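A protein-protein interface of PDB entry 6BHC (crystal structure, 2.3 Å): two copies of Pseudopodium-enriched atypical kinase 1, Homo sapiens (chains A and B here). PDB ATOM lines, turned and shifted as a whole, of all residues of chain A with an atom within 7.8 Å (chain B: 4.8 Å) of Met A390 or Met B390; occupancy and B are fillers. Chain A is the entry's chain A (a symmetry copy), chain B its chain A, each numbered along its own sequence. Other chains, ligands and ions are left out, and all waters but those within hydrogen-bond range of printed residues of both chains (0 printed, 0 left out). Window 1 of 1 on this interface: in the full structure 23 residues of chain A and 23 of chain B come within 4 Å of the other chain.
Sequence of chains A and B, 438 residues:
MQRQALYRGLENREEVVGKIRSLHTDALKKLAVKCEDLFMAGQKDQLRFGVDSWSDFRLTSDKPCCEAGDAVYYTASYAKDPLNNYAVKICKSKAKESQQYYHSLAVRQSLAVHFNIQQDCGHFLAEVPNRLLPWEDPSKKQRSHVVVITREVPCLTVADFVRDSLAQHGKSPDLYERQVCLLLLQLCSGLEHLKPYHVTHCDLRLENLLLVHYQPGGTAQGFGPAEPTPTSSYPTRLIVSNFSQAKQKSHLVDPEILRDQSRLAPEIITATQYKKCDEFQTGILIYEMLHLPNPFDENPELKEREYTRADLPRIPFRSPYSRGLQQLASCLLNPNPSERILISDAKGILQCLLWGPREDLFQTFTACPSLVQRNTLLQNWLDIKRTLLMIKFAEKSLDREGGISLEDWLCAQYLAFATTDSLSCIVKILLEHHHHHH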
ATOM      1  N   LEU A  23     -11.349  -5.170 -28.289  1.00  0.00           N
ATOM      2  CA  LEU A  23     -10.574  -5.584 -27.124  1.00  0.00           C
ATOM      3  C   LEU A  23     -10.392  -4.432 -26.146  1.00  0.00           C
ATOM      4  O   LEU A  23     -10.590  -4.595 -24.937  1.00  0.00           O
ATOM      5  CB  LEU A  23      -9.217  -6.136 -27.563  1.00  0.00           C
ATOM      6  CG  LEU A  23      -9.210  -7.511 -28.230  1.00  0.00           C
ATOM      7  CD1 LEU A  23      -7.816  -7.851 -28.728  1.00  0.00           C
ATOM      8  CD2 LEU A  23      -9.711  -8.573 -27.264  1.00  0.00           C
ATOM      9  N   HIS A  24     -10.008  -3.258 -26.650  1.00  0.00           N
ATOM     10  CA  HIS A  24      -9.829  -2.102 -25.777  1.00  0.00           C
ATOM     11  C   HIS A  24     -11.142  -1.699 -25.122  1.00  0.00           C
ATOM     12  O   HIS A  24     -11.174  -1.375 -23.929  1.00  0.00           O
ATOM     13  CB  HIS A  24      -9.244  -0.931 -26.566  1.00  0.00           C
ATOM     14  CG  HIS A  24      -7.752  -0.960 -26.671  1.00  0.00           C
ATOM     15  ND1 HIS A  24      -7.075  -0.524 -27.790  1.00  0.00           N
ATOM     16  CD2 HIS A  24      -6.805  -1.366 -25.792  1.00  0.00           C
ATOM     17  CE1 HIS A  24      -5.776  -0.666 -27.598  1.00  0.00           C
ATOM     18  NE2 HIS A  24      -5.585  -1.174 -26.394  1.00  0.00           N
ATOM     19  N   THR A  25     -12.234  -1.720 -25.886  1.00  0.00           N
ATOM     20  CA  THR A  25     -13.527  -1.309 -25.348  1.00  0.00           C
ATOM     21  C   THR A  25     -13.988  -2.252 -24.243  1.00  0.00           C
ATOM     22  O   THR A  25     -14.411  -1.809 -23.169  1.00  0.00           O
ATOM     23  CB  THR A  25     -14.559  -1.242 -26.473  1.00  0.00           C
ATOM     24  OG1 THR A  25     -14.153  -0.260 -27.435  1.00  0.00           O
ATOM     25  CG2 THR A  25     -15.926  -0.871 -25.925  1.00  0.00           C
ATOM     26  N   ASP A  26     -13.903  -3.563 -24.486  1.00  0.00           N
ATOM     27  CA  ASP A  26     -14.297  -4.526 -23.463  1.00  0.00           C
ATOM     28  C   ASP A  26     -13.370  -4.476 -22.255  1.00  0.00           C
ATOM     29  O   ASP A  26     -13.820  -4.684 -21.123  1.00  0.00           O
ATOM     30  CB  ASP A  26     -14.327  -5.938 -24.050  1.00  0.00           C
ATOM     31  CG  ASP A  26     -15.324  -6.077 -25.186  1.00  0.00           C
ATOM     32  OD1 ASP A  26     -16.274  -5.268 -25.250  1.00  0.00           O
ATOM     33  OD2 ASP A  26     -15.159  -7.001 -26.012  1.00  0.00           O
ATOM     34  N   ALA A  27     -12.082  -4.198 -22.469  1.00  0.00           N
ATOM     35  CA  ALA A  27     -11.148  -4.118 -21.351  1.00  0.00           C
ATOM     36  C   ALA A  27     -11.427  -2.894 -20.486  1.00  0.00           C
ATOM     37  O   ALA A  27     -11.428  -2.983 -19.252  1.00  0.00           O
ATOM     38  CB  ALA A  27      -9.709  -4.099 -21.865  1.00  0.00           C
ATOM     39  N   LEU A  28     -11.666  -1.740 -21.115  1.00  0.00           N
ATOM     40  CA  LEU A  28     -11.931  -0.524 -20.349  1.00  0.00           C
ATOM     41  C   LEU A  28     -13.228  -0.629 -19.559  1.00  0.00           C
ATOM     42  O   LEU A  28     -13.332  -0.067 -18.462  1.00  0.00           O
ATOM     43  CB  LEU A  28     -11.971   0.690 -21.278  1.00  0.00           C
ATOM     44  CG  LEU A  28     -10.623   1.239 -21.752  1.00  0.00           C
ATOM     45  CD1 LEU A  28     -10.830   2.391 -22.717  1.00  0.00           C
ATOM     46  CD2 LEU A  28      -9.777   1.682 -20.566  1.00  0.00           C
ATOM     47  N   LYS A  29     -14.226  -1.335 -20.094  1.00  0.00           N
ATOM     48  CA  LYS A  29     -15.443  -1.581 -19.328  1.00  0.00           C
ATOM     49  C   LYS A  29     -15.157  -2.451 -18.111  1.00  0.00           C
ATOM     50  O   LYS A  29     -15.715  -2.221 -17.032  1.00  0.00           O
ATOM     51  CB  LYS A  29     -16.506  -2.229 -20.214  1.00  0.00           C
ATOM     52  CG  LYS A  29     -17.068  -1.305 -21.278  1.00  0.00           C
ATOM     53  CD  LYS A  29     -18.069  -2.026 -22.161  1.00  0.00           C
ATOM     54  CE  LYS A  29     -18.629  -1.096 -23.221  1.00  0.00           C
ATOM     55  NZ  LYS A  29     -19.474  -1.829 -24.201  1.00  0.00           N
ATOM     56  N   LEU A  31     -12.213  -2.639 -16.580  1.00  0.00           N
ATOM     57  CA  LEU A  31     -11.443  -1.801 -15.667  1.00  0.00           C
ATOM     58  C   LEU A  31     -12.344  -0.827 -14.919  1.00  0.00           C
ATOM     59  O   LEU A  31     -12.135  -0.569 -13.727  1.00  0.00           O
ATOM     60  CB  LEU A  31     -10.359  -1.045 -16.437  1.00  0.00           C
ATOM     61  CG  LEU A  31      -9.227  -1.883 -17.032  1.00  0.00           C
ATOM     62  CD1 LEU A  31      -8.375  -1.045 -17.977  1.00  0.00           C
ATOM     63  CD2 LEU A  31      -8.371  -2.481 -15.927  1.00  0.00           C
ATOM     64  N   ILE A 384      -7.168   6.304 -30.270  1.00  0.00           N
ATOM     65  CA  ILE A 384      -5.931   6.817 -29.692  1.00  0.00           C
ATOM     66  C   ILE A 384      -6.093   7.058 -28.196  1.00  0.00           C
ATOM     67  O   ILE A 384      -5.220   6.697 -27.399  1.00  0.00           O
ATOM     68  CB  ILE A 384      -5.492   8.095 -30.429  1.00  0.00           C
ATOM     69  CG1 ILE A 384      -5.121   7.771 -31.877  1.00  0.00           C
ATOM     70  CG2 ILE A 384      -4.328   8.760 -29.709  1.00  0.00           C
ATOM     71  CD1 ILE A 384      -4.682   8.977 -32.681  1.00  0.00           C
ATOM     72  N   LYS A 385      -7.210   7.668 -27.791  1.00  0.00           N
ATOM     73  CA  LYS A 385      -7.424   7.956 -26.376  1.00  0.00           C
ATOM     74  C   LYS A 385      -7.571   6.677 -25.562  1.00  0.00           C
ATOM     75  O   LYS A 385      -7.080   6.598 -24.430  1.00  0.00           O
ATOM     76  CB  LYS A 385      -8.653   8.849 -26.199  1.00  0.00           C
ATOM     77  CG  LYS A 385      -8.464  10.264 -26.718  1.00  0.00           C
ATOM     78  CD  LYS A 385      -7.588  11.092 -25.790  1.00  0.00           C
ATOM     79  CE  LYS A 385      -8.278  11.328 -24.454  1.00  0.00           C
ATOM     80  NZ  LYS A 385      -7.487  12.218 -23.558  1.00  0.00           N
ATOM     81  N   ARG A 386      -8.242   5.664 -26.118  1.00  0.00           N
ATOM     82  CA  ARG A 386      -8.356   4.390 -25.415  1.00  0.00           C
ATOM     83  C   ARG A 386      -6.993   3.729 -25.260  1.00  0.00           C
ATOM     84  O   ARG A 386      -6.707   3.106 -24.230  1.00  0.00           O
ATOM     85  CB  ARG A 386      -9.320   3.460 -26.151  1.00  0.00           C
ATOM     86  CG  ARG A 386     -10.776   3.886 -26.086  1.00  0.00           C
ATOM     87  CD  ARG A 386     -11.686   2.741 -26.497  1.00  0.00           C
ATOM     88  NE  ARG A 386     -13.098   3.094 -26.410  1.00  0.00           N
ATOM     89  CZ  ARG A 386     -13.892   3.267 -27.462  1.00  0.00           C
ATOM     90  NH1 ARG A 386     -13.413   3.113 -28.688  1.00  0.00           N
ATOM     91  NH2 ARG A 386     -15.167   3.586 -27.287  1.00  0.00           N
ATOM     92  N   THR A 387      -6.139   3.854 -26.278  1.00  0.00           N
ATOM     93  CA  THR A 387      -4.793   3.297 -26.192  1.00  0.00           C
ATOM     94  C   THR A 387      -3.970   4.010 -25.127  1.00  0.00           C
ATOM     95  O   THR A 387      -3.274   3.363 -24.336  1.00  0.00           O
ATOM     96  CB  THR A 387      -4.104   3.384 -27.555  1.00  0.00           C
ATOM     97  OG1 THR A 387      -4.878   2.671 -28.528  1.00  0.00           O
ATOM     98  CG2 THR A 387      -2.707   2.788 -27.491  1.00  0.00           C
ATOM     99  N   LEU A 388      -4.045   5.342 -25.087  1.00  0.00           N
ATOM    100  CA  LEU A 388      -3.293   6.103 -24.094  1.00  0.00           C
ATOM    101  C   LEU A 388      -3.734   5.750 -22.678  1.00  0.00           C
ATOM    102  O   LEU A 388      -2.898   5.530 -21.793  1.00  0.00           O
ATOM    103  CB  LEU A 388      -3.457   7.601 -24.353  1.00  0.00           C
ATOM    104  CG  LEU A 388      -2.794   8.128 -25.626  1.00  0.00           C
ATOM    105  CD1 LEU A 388      -3.144   9.591 -25.851  1.00  0.00           C
ATOM    106  CD2 LEU A 388      -1.289   7.940 -25.547  1.00  0.00           C
ATOM    107  N   LEU A 389      -5.046   5.689 -22.446  1.00  0.00           N
ATOM    108  CA  LEU A 389      -5.540   5.364 -21.111  1.00  0.00           C
ATOM    109  C   LEU A 389      -5.157   3.945 -20.712  1.00  0.00           C
ATOM    110  O   LEU A 389      -4.806   3.693 -19.552  1.00  0.00           O
ATOM    111  CB  LEU A 389      -7.055   5.549 -21.049  1.00  0.00           C
ATOM    112  CG  LEU A 389      -7.683   5.310 -19.672  1.00  0.00           C
ATOM    113  CD1 LEU A 389      -7.070   6.241 -18.636  1.00  0.00           C
ATOM    114  CD2 LEU A 389      -9.189   5.487 -19.728  1.00  0.00           C
ATOM    115  N   MET A 390      -5.213   3.003 -21.658  1.00  0.00           N
ATOM    116  CA  MET A 390      -4.812   1.633 -21.356  1.00  0.00           C
ATOM    117  C   MET A 390      -3.342   1.568 -20.962  1.00  0.00           C
ATOM    118  O   MET A 390      -2.969   0.831 -20.042  1.00  0.00           O
ATOM    119  CB  MET A 390      -5.087   0.727 -22.556  1.00  0.00           C
ATOM    120  CG  MET A 390      -4.945  -0.758 -22.260  1.00  0.00           C
ATOM    121  SD  MET A 390      -6.239  -1.363 -21.159  1.00  0.00           S
ATOM    122  CE  MET A 390      -7.700  -0.975 -22.118  1.00  0.00           C
ATOM    123  N   ILE A 391      -2.493   2.334 -21.651  1.00  0.00           N
ATOM    124  CA  ILE A 391      -1.079   2.395 -21.292  1.00  0.00           C
ATOM    125  C   ILE A 391      -0.910   2.965 -19.890  1.00  0.00           C
ATOM    126  O   ILE A 391      -0.077   2.492 -19.108  1.00  0.00           O
ATOM    127  CB  ILE A 391      -0.304   3.216 -22.341  1.00  0.00           C
ATOM    128  CG1 ILE A 391      -0.278   2.480 -23.682  1.00  0.00           C
ATOM    129  CG2 ILE A 391       1.111   3.516 -21.862  1.00  0.00           C
ATOM    130  CD1 ILE A 391       0.283   3.306 -24.823  1.00  0.00           C
ATOM    131  N   LYS A 392      -1.711   3.978 -19.544  1.00  0.00           N
ATOM    132  CA  LYS A 392      -1.611   4.594 -18.224  1.00  0.00           C
ATOM    133  C   LYS A 392      -1.903   3.589 -17.117  1.00  0.00           C
ATOM    134  O   LYS A 392      -1.191   3.541 -16.108  1.00  0.00           O
ATOM    135  CB  LYS A 392      -2.564   5.785 -18.130  1.00  0.00           C
ATOM    136  CG  LYS A 392      -2.530   6.514 -16.793  1.00  0.00           C
ATOM    137  CD  LYS A 392      -3.657   7.534 -16.701  1.00  0.00           C
ATOM    138  CE  LYS A 392      -3.600   8.321 -15.401  1.00  0.00           C
ATOM    139  NZ  LYS A 392      -2.388   9.179 -15.319  1.00  0.00           N
ATOM    140  N   PHE A 393      -2.950   2.776 -17.286  1.00  0.00           N
ATOM    141  CA  PHE A 393      -3.259   1.759 -16.287  1.00  0.00           C
ATOM    142  C   PHE A 393      -2.152   0.717 -16.204  1.00  0.00           C
ATOM    143  O   PHE A 393      -1.800   0.260 -15.110  1.00  0.00           O
ATOM    144  CB  PHE A 393      -4.597   1.091 -16.602  1.00  0.00           C
ATOM    145  CG  PHE A 393      -5.784   1.807 -16.025  1.00  0.00           C
ATOM    146  CD1 PHE A 393      -6.219   1.528 -14.738  1.00  0.00           C
ATOM    147  CD2 PHE A 393      -6.466   2.755 -16.768  1.00  0.00           C
ATOM    148  CE1 PHE A 393      -7.314   2.185 -14.204  1.00  0.00           C
ATOM    149  CE2 PHE A 393      -7.561   3.416 -16.241  1.00  0.00           C
ATOM    150  CZ  PHE A 393      -7.985   3.130 -14.956  1.00  0.00           C
ATOM    151  N   ALA A 394      -1.586   0.334 -17.351  1.00  0.00           N
ATOM    152  CA  ALA A 394      -0.532  -0.674 -17.365  1.00  0.00           C
ATOM    153  C   ALA A 394       0.715  -0.187 -16.637  1.00  0.00           C
ATOM    154  O   ALA A 394       1.403  -0.974 -15.976  1.00  0.00           O
ATOM    155  CB  ALA A 394      -0.197  -1.061 -18.806  1.00  0.00           C
ATOM    156  N   GLU A 395       1.025   1.108 -16.747  1.00  0.00           N
ATOM    157  CA  GLU A 395       2.210   1.639 -16.082  1.00  0.00           C
ATOM    158  C   GLU A 395       2.022   1.715 -14.571  1.00  0.00           C
ATOM    159  O   GLU A 395       3.002   1.624 -13.821  1.00  0.00           O
ATOM    160  CB  GLU A 395       2.562   3.015 -16.648  1.00  0.00           C
ATOM    161  CG  GLU A 395       2.895   3.001 -18.136  1.00  0.00           C
ATOM    162  CD  GLU A 395       3.301   4.366 -18.664  1.00  0.00           C
ATOM    163  OE1 GLU A 395       4.277   4.439 -19.439  1.00  0.00           O
ATOM    164  OE2 GLU A 395       2.646   5.365 -18.301  1.00  0.00           O
ATOM    165  N   LYS A 396       0.782   1.876 -14.102  1.00  0.00           N
ATOM    166  CA  LYS A 396       0.542   1.897 -12.665  1.00  0.00           C
ATOM    167  C   LYS A 396       0.705   0.522 -12.029  1.00  0.00           C
ATOM    168  O   LYS A 396       0.891   0.438 -10.811  1.00  0.00           O
ATOM    169  CB  LYS A 396      -0.852   2.451 -12.365  1.00  0.00           C
ATOM    170  CG  LYS A 396      -0.932   3.966 -12.431  1.00  0.00           C
ATOM    171  CD  LYS A 396      -2.305   4.471 -12.023  1.00  0.00           C
ATOM    172  CE  LYS A 396      -2.302   5.980 -11.844  1.00  0.00           C
ATOM    173  NZ  LYS A 396      -1.343   6.407 -10.787  1.00  0.00           N
ATOM    174  N   SER A 397       0.653  -0.552 -12.820  1.00  0.00           N
ATOM    175  CA  SER A 397       0.856  -1.889 -12.275  1.00  0.00           C
ATOM    176  C   SER A 397       2.284  -2.116 -11.797  1.00  0.00           C
ATOM    177  O   SER A 397       2.534  -3.105 -11.099  1.00  0.00           O
ATOM    178  CB  SER A 397       0.489  -2.948 -13.317  1.00  0.00           C
ATOM    179  OG  SER A 397       1.409  -2.950 -14.396  1.00  0.00           O
ATOM    180  N   LEU A 415     -14.398   6.726 -21.722  1.00  0.00           N
ATOM    181  CA  LEU A 415     -13.882   6.108 -22.940  1.00  0.00           C
ATOM    182  C   LEU A 415     -14.444   4.710 -23.164  1.00  0.00           C
ATOM    183  O   LEU A 415     -14.520   4.253 -24.310  1.00  0.00           O
ATOM    184  CB  LEU A 415     -12.356   6.062 -22.898  1.00  0.00           C
ATOM    185  CG  LEU A 415     -11.675   7.430 -22.821  1.00  0.00           C
ATOM    186  CD1 LEU A 415     -10.166   7.287 -22.898  1.00  0.00           C
ATOM    187  CD2 LEU A 415     -12.193   8.340 -23.924  1.00  0.00           C
ATOM    188  N   HIS B  24       1.943   1.423 -28.545  1.00  0.00           N
ATOM    189  CA  HIS B  24       2.061   0.140 -27.861  1.00  0.00           C
ATOM    190  C   HIS B  24       3.510  -0.322 -27.804  1.00  0.00           C
ATOM    191  O   HIS B  24       3.967  -0.829 -26.772  1.00  0.00           O
ATOM    192  CB  HIS B  24       1.194  -0.909 -28.555  1.00  0.00           C
ATOM    193  CG  HIS B  24      -0.232  -0.910 -28.101  1.00  0.00           C
ATOM    194  ND1 HIS B  24      -1.284  -1.184 -28.949  1.00  0.00           N
ATOM    195  CD2 HIS B  24      -0.779  -0.676 -26.885  1.00  0.00           C
ATOM    196  CE1 HIS B  24      -2.419  -1.113 -28.275  1.00  0.00           C
ATOM    197  NE2 HIS B  24      -2.140  -0.807 -27.021  1.00  0.00           N
ATOM    198  N   ALA B  27       5.429   1.754 -25.320  1.00  0.00           N
ATOM    199  CA  ALA B  27       4.968   1.470 -23.965  1.00  0.00           C
ATOM    200  C   ALA B  27       5.506   0.134 -23.467  1.00  0.00           C
ATOM    201  O   ALA B  27       5.962   0.027 -22.322  1.00  0.00           O
ATOM    202  CB  ALA B  27       3.441   1.490 -23.913  1.00  0.00           C
ATOM    203  N   LEU B  28       5.464  -0.899 -24.313  1.00  0.00           N
ATOM    204  CA  LEU B  28       5.954  -2.211 -23.900  1.00  0.00           C
ATOM    205  C   LEU B  28       7.453  -2.194 -23.633  1.00  0.00           C
ATOM    206  O   LEU B  28       7.934  -2.918 -22.754  1.00  0.00           O
ATOM    207  CB  LEU B  28       5.615  -3.261 -24.958  1.00  0.00           C
ATOM    208  CG  LEU B  28       4.171  -3.770 -24.986  1.00  0.00           C
ATOM    209  CD1 LEU B  28       3.976  -4.748 -26.129  1.00  0.00           C
ATOM    210  CD2 LEU B  28       3.805  -4.420 -23.659  1.00  0.00           C
ATOM    211  N   LEU B  31       7.659  -0.711 -20.212  1.00  0.00           N
ATOM    212  CA  LEU B  31       7.251  -1.705 -19.225  1.00  0.00           C
ATOM    213  C   LEU B  31       8.334  -2.758 -19.022  1.00  0.00           C
ATOM    214  O   LEU B  31       8.568  -3.206 -17.894  1.00  0.00           O
ATOM    215  CB  LEU B  31       5.939  -2.362 -19.654  1.00  0.00           C
ATOM    216  CG  LEU B  31       4.693  -1.475 -19.654  1.00  0.00           C
ATOM    217  CD1 LEU B  31       3.530  -2.178 -20.341  1.00  0.00           C
ATOM    218  CD2 LEU B  31       4.318  -1.085 -18.233  1.00  0.00           C
ATOM    219  N   ARG B 386       0.227  -7.520 -28.819  1.00  0.00           N
ATOM    220  CA  ARG B 386       0.628  -6.370 -28.014  1.00  0.00           C
ATOM    221  C   ARG B 386      -0.563  -5.782 -27.270  1.00  0.00           C
ATOM    222  O   ARG B 386      -0.434  -5.339 -26.122  1.00  0.00           O
ATOM    223  CB  ARG B 386       1.284  -5.307 -28.896  1.00  0.00           C
ATOM    224  CG  ARG B 386       2.649  -5.693 -29.436  1.00  0.00           C
ATOM    225  CD  ARG B 386       3.379  -4.471 -29.965  1.00  0.00           C
ATOM    226  NE  ARG B 386       4.714  -4.790 -30.457  1.00  0.00           N
ATOM    227  CZ  ARG B 386       5.063  -4.772 -31.740  1.00  0.00           C
ATOM    228  NH1 ARG B 386       4.174  -4.441 -32.665  1.00  0.00           N
ATOM    229  NH2 ARG B 386       6.303  -5.075 -32.096  1.00  0.00           N
ATOM    230  N   THR B 387      -1.734  -5.771 -27.911  1.00  0.00           N
ATOM    231  CA  THR B 387      -2.938  -5.275 -27.252  1.00  0.00           C
ATOM    232  C   THR B 387      -3.336  -6.172 -26.087  1.00  0.00           C
ATOM    233  O   THR B 387      -3.674  -5.680 -25.004  1.00  0.00           O
ATOM    234  CB  THR B 387      -4.080  -5.167 -28.263  1.00  0.00           C
ATOM    235  OG1 THR B 387      -3.694  -4.286 -29.326  1.00  0.00           O
ATOM    236  CG2 THR B 387      -5.338  -4.631 -27.600  1.00  0.00           C
ATOM    237  N   LEU B 388      -3.292  -7.491 -26.287  1.00  0.00           N
ATOM    238  CA  LEU B 388      -3.651  -8.422 -25.222  1.00  0.00           C
ATOM    239  C   LEU B 388      -2.712  -8.284 -24.028  1.00  0.00           C
ATOM    240  O   LEU B 388      -3.159  -8.231 -22.876  1.00  0.00           O
ATOM    241  CB  LEU B 388      -3.638  -9.854 -25.755  1.00  0.00           C
ATOM    242  CG  LEU B 388      -4.736 -10.193 -26.763  1.00  0.00           C
ATOM    243  CD1 LEU B 388      -4.537 -11.591 -27.329  1.00  0.00           C
ATOM    244  CD2 LEU B 388      -6.102 -10.065 -26.111  1.00  0.00           C
ATOM    245  N   LEU B 389      -1.404  -8.220 -24.286  1.00  0.00           N
ATOM    246  CA  LEU B 389      -0.447  -8.095 -23.191  1.00  0.00           C
ATOM    247  C   LEU B 389      -0.614  -6.769 -22.460  1.00  0.00           C
ATOM    248  O   LEU B 389      -0.509  -6.714 -21.229  1.00  0.00           O
ATOM    249  CB  LEU B 389       0.980  -8.242 -23.717  1.00  0.00           C
ATOM    250  CG  LEU B 389       2.074  -8.204 -22.646  1.00  0.00           C
ATOM    251  CD1 LEU B 389       1.855  -9.306 -21.618  1.00  0.00           C
ATOM    252  CD2 LEU B 389       3.450  -8.325 -23.276  1.00  0.00           C
ATOM    253  N   MET B 390      -0.880  -5.689 -23.200  1.00  0.00           N
ATOM    254  CA  MET B 390      -1.101  -4.396 -22.560  1.00  0.00           C
ATOM    255  C   MET B 390      -2.323  -4.438 -21.651  1.00  0.00           C
ATOM    256  O   MET B 390      -2.311  -3.867 -20.555  1.00  0.00           O
ATOM    257  CB  MET B 390      -1.257  -3.305 -23.618  1.00  0.00           C
ATOM    258  CG  MET B 390      -1.236  -1.890 -23.060  1.00  0.00           C
ATOM    259  SD  MET B 390       0.388  -1.427 -22.428  1.00  0.00           S
ATOM    260  CE  MET B 390       1.385  -1.614 -23.903  1.00  0.00           C
ATOM    261  N   ILE B 391      -3.387  -5.111 -22.093  1.00  0.00           N
ATOM    262  CA  ILE B 391      -4.574  -5.270 -21.257  1.00  0.00           C
ATOM    263  C   ILE B 391      -4.235  -6.059 -19.998  1.00  0.00           C
ATOM    264  O   ILE B 391      -4.710  -5.741 -18.902  1.00  0.00           O
ATOM    265  CB  ILE B 391      -5.703  -5.939 -22.065  1.00  0.00           C
ATOM    266  CG1 ILE B 391      -6.196  -5.001 -23.169  1.00  0.00           C
ATOM    267  CG2 ILE B 391      -6.853  -6.352 -21.155  1.00  0.00           C
ATOM    268  CD1 ILE B 391      -7.160  -5.653 -24.141  1.00  0.00           C
ATOM    269  N   LYS B 392      -3.394  -7.089 -20.134  1.00  0.00           N
ATOM    270  CA  LYS B 392      -3.023  -7.910 -18.984  1.00  0.00           C
ATOM    271  C   LYS B 392      -2.316  -7.083 -17.917  1.00  0.00           C
ATOM    272  O   LYS B 392      -2.608  -7.217 -16.723  1.00  0.00           O
ATOM    273  CB  LYS B 392      -2.138  -9.071 -19.434  1.00  0.00           C
ATOM    274  CG  LYS B 392      -1.702 -10.002 -18.311  1.00  0.00           C
ATOM    275  CD  LYS B 392      -0.651 -10.990 -18.799  1.00  0.00           C
ATOM    276  CE  LYS B 392      -0.252 -11.973 -17.710  1.00  0.00           C
ATOM    277  NZ  LYS B 392      -1.375 -12.870 -17.328  1.00  0.00           N
ATOM    278  N   PHE B 393      -1.379  -6.223 -18.327  1.00  0.00           N
ATOM    279  CA  PHE B 393      -0.696  -5.367 -17.362  1.00  0.00           C
ATOM    280  C   PHE B 393      -1.664  -4.385 -16.717  1.00  0.00           C
ATOM    281  O   PHE B 393      -1.578  -4.117 -15.512  1.00  0.00           O
ATOM    282  CB  PHE B 393       0.454  -4.618 -18.036  1.00  0.00           C
ATOM    283  CG  PHE B 393       1.747  -5.380 -18.053  1.00  0.00           C
ATOM    284  CD1 PHE B 393       2.631  -5.294 -16.988  1.00  0.00           C
ATOM    285  CD2 PHE B 393       2.082  -6.178 -19.135  1.00  0.00           C
ATOM    286  CE1 PHE B 393       3.826  -5.994 -17.002  1.00  0.00           C
ATOM    287  CE2 PHE B 393       3.273  -6.880 -19.155  1.00  0.00           C
ATOM    288  CZ  PHE B 393       4.146  -6.788 -18.087  1.00  0.00           C
ATOM    289  N   ALA B 394      -2.598  -3.843 -17.502  1.00  0.00           N
ATOM    290  CA  ALA B 394      -3.553  -2.878 -16.970  1.00  0.00           C
ATOM    291  C   ALA B 394      -4.462  -3.511 -15.923  1.00  0.00           C
ATOM    292  O   ALA B 394      -4.837  -2.859 -14.941  1.00  0.00           O
ATOM    293  CB  ALA B 394      -4.380  -2.279 -18.108  1.00  0.00           C
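Printed residues of chain B within 4 Å of Met A390: Met B390 and Ala B394.
Of the printed residues of chain A, Leu B31 touches Ala A394 (3.7 Å).
Printed residues of chain B within 4 Å of Leu A23: Leu B388 and Ile B391.
Printed residues of chain A within 4 Å of Ala B27: Ile A391.
Printed residues of chain B within 4 Å of Leu A31: Ala B394 (3.7 Å).
Lys A392 touches none of the printed residues of chain B.
Asp A26 touches none of the printed residues of chain B.
The nearest residue of chain B that does not touch Met A390 is Ile B391 (4.2 Å).
The nearest residue of chain A that does not touch Met B390 is Ile A391 (4.2 Å).
Of the 13 printed residues of chain B, 9 touch a printed residue of chain A.
Hydrophobic or aromatic side chains of chain B that line the printed part of chain A: His B24, Ala B27, Leu B31, Leu B388, Met B390, Ile B391, Phe B393 and Ala B394.
Of the 23 printed residues of chain A, 10 touch a printed residue of chain B.
Hydrophobic or aromatic side chains of chain A within 4 Å of the printed part of chain B: Leu A23, His A24, Ala A27, Leu A31, Met A390, Ile A391, Phe A393 and Ala A394.
Among the printed residues, no Asp or Glu carboxylate lies within 4 Å of a Lys or Arg side-chain nitrogen of the other chain.
OG of Ser A397 lies within hydrogen-bond range of O of Ala A394 (2.5 Å).
His B24 touches its own counterpart, His A24.
His A24 touches Thr B387, and with the chains exchanged Thr A387 touches His B24.
Leu A31 touches Ala B394, and with the chains exchanged Ala A394 touches Leu B31.
Ala B394 touches its own counterpart, Ala A394.
Of the 16 pairs that touch across the chains among the printed residues, 13 have their exchanged pair printed and touching as well.
The backbone carbonyl oxygen (O) of Phe B393 lies close to the side-chain hydroxyl (OG) of Ser A397, at 3.4 Å.
Among the printed residues, merely in contact across the chains: Leu A23 with Leu B388 (3.8 Å), Leu A23 with Ile B391 (3.7 Å), His A24 with His B24 (3.5 Å), His A24 with Thr B387 (3.7 Å), Ala A27 with Ile B391 (3.7 Å), Leu A31 with Ala B394 (3.7 Å), Thr A387 with His B24 (3.7 Å), Met A390 with Met B390 (3.96 Å), Met A390 with Ala B394 (3.7 Å), Ile A391 with Ala B27 (3.7 Å), Phe A393 with Ala B394 (3.7 Å), Ala A394 with Leu B31 (3.7 Å), Ala A394 with Met B390 (3.7 Å), Ala A394 with Phe B393 (3.7 Å) and Ala A394 with Ala B394 (3.8 Å).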
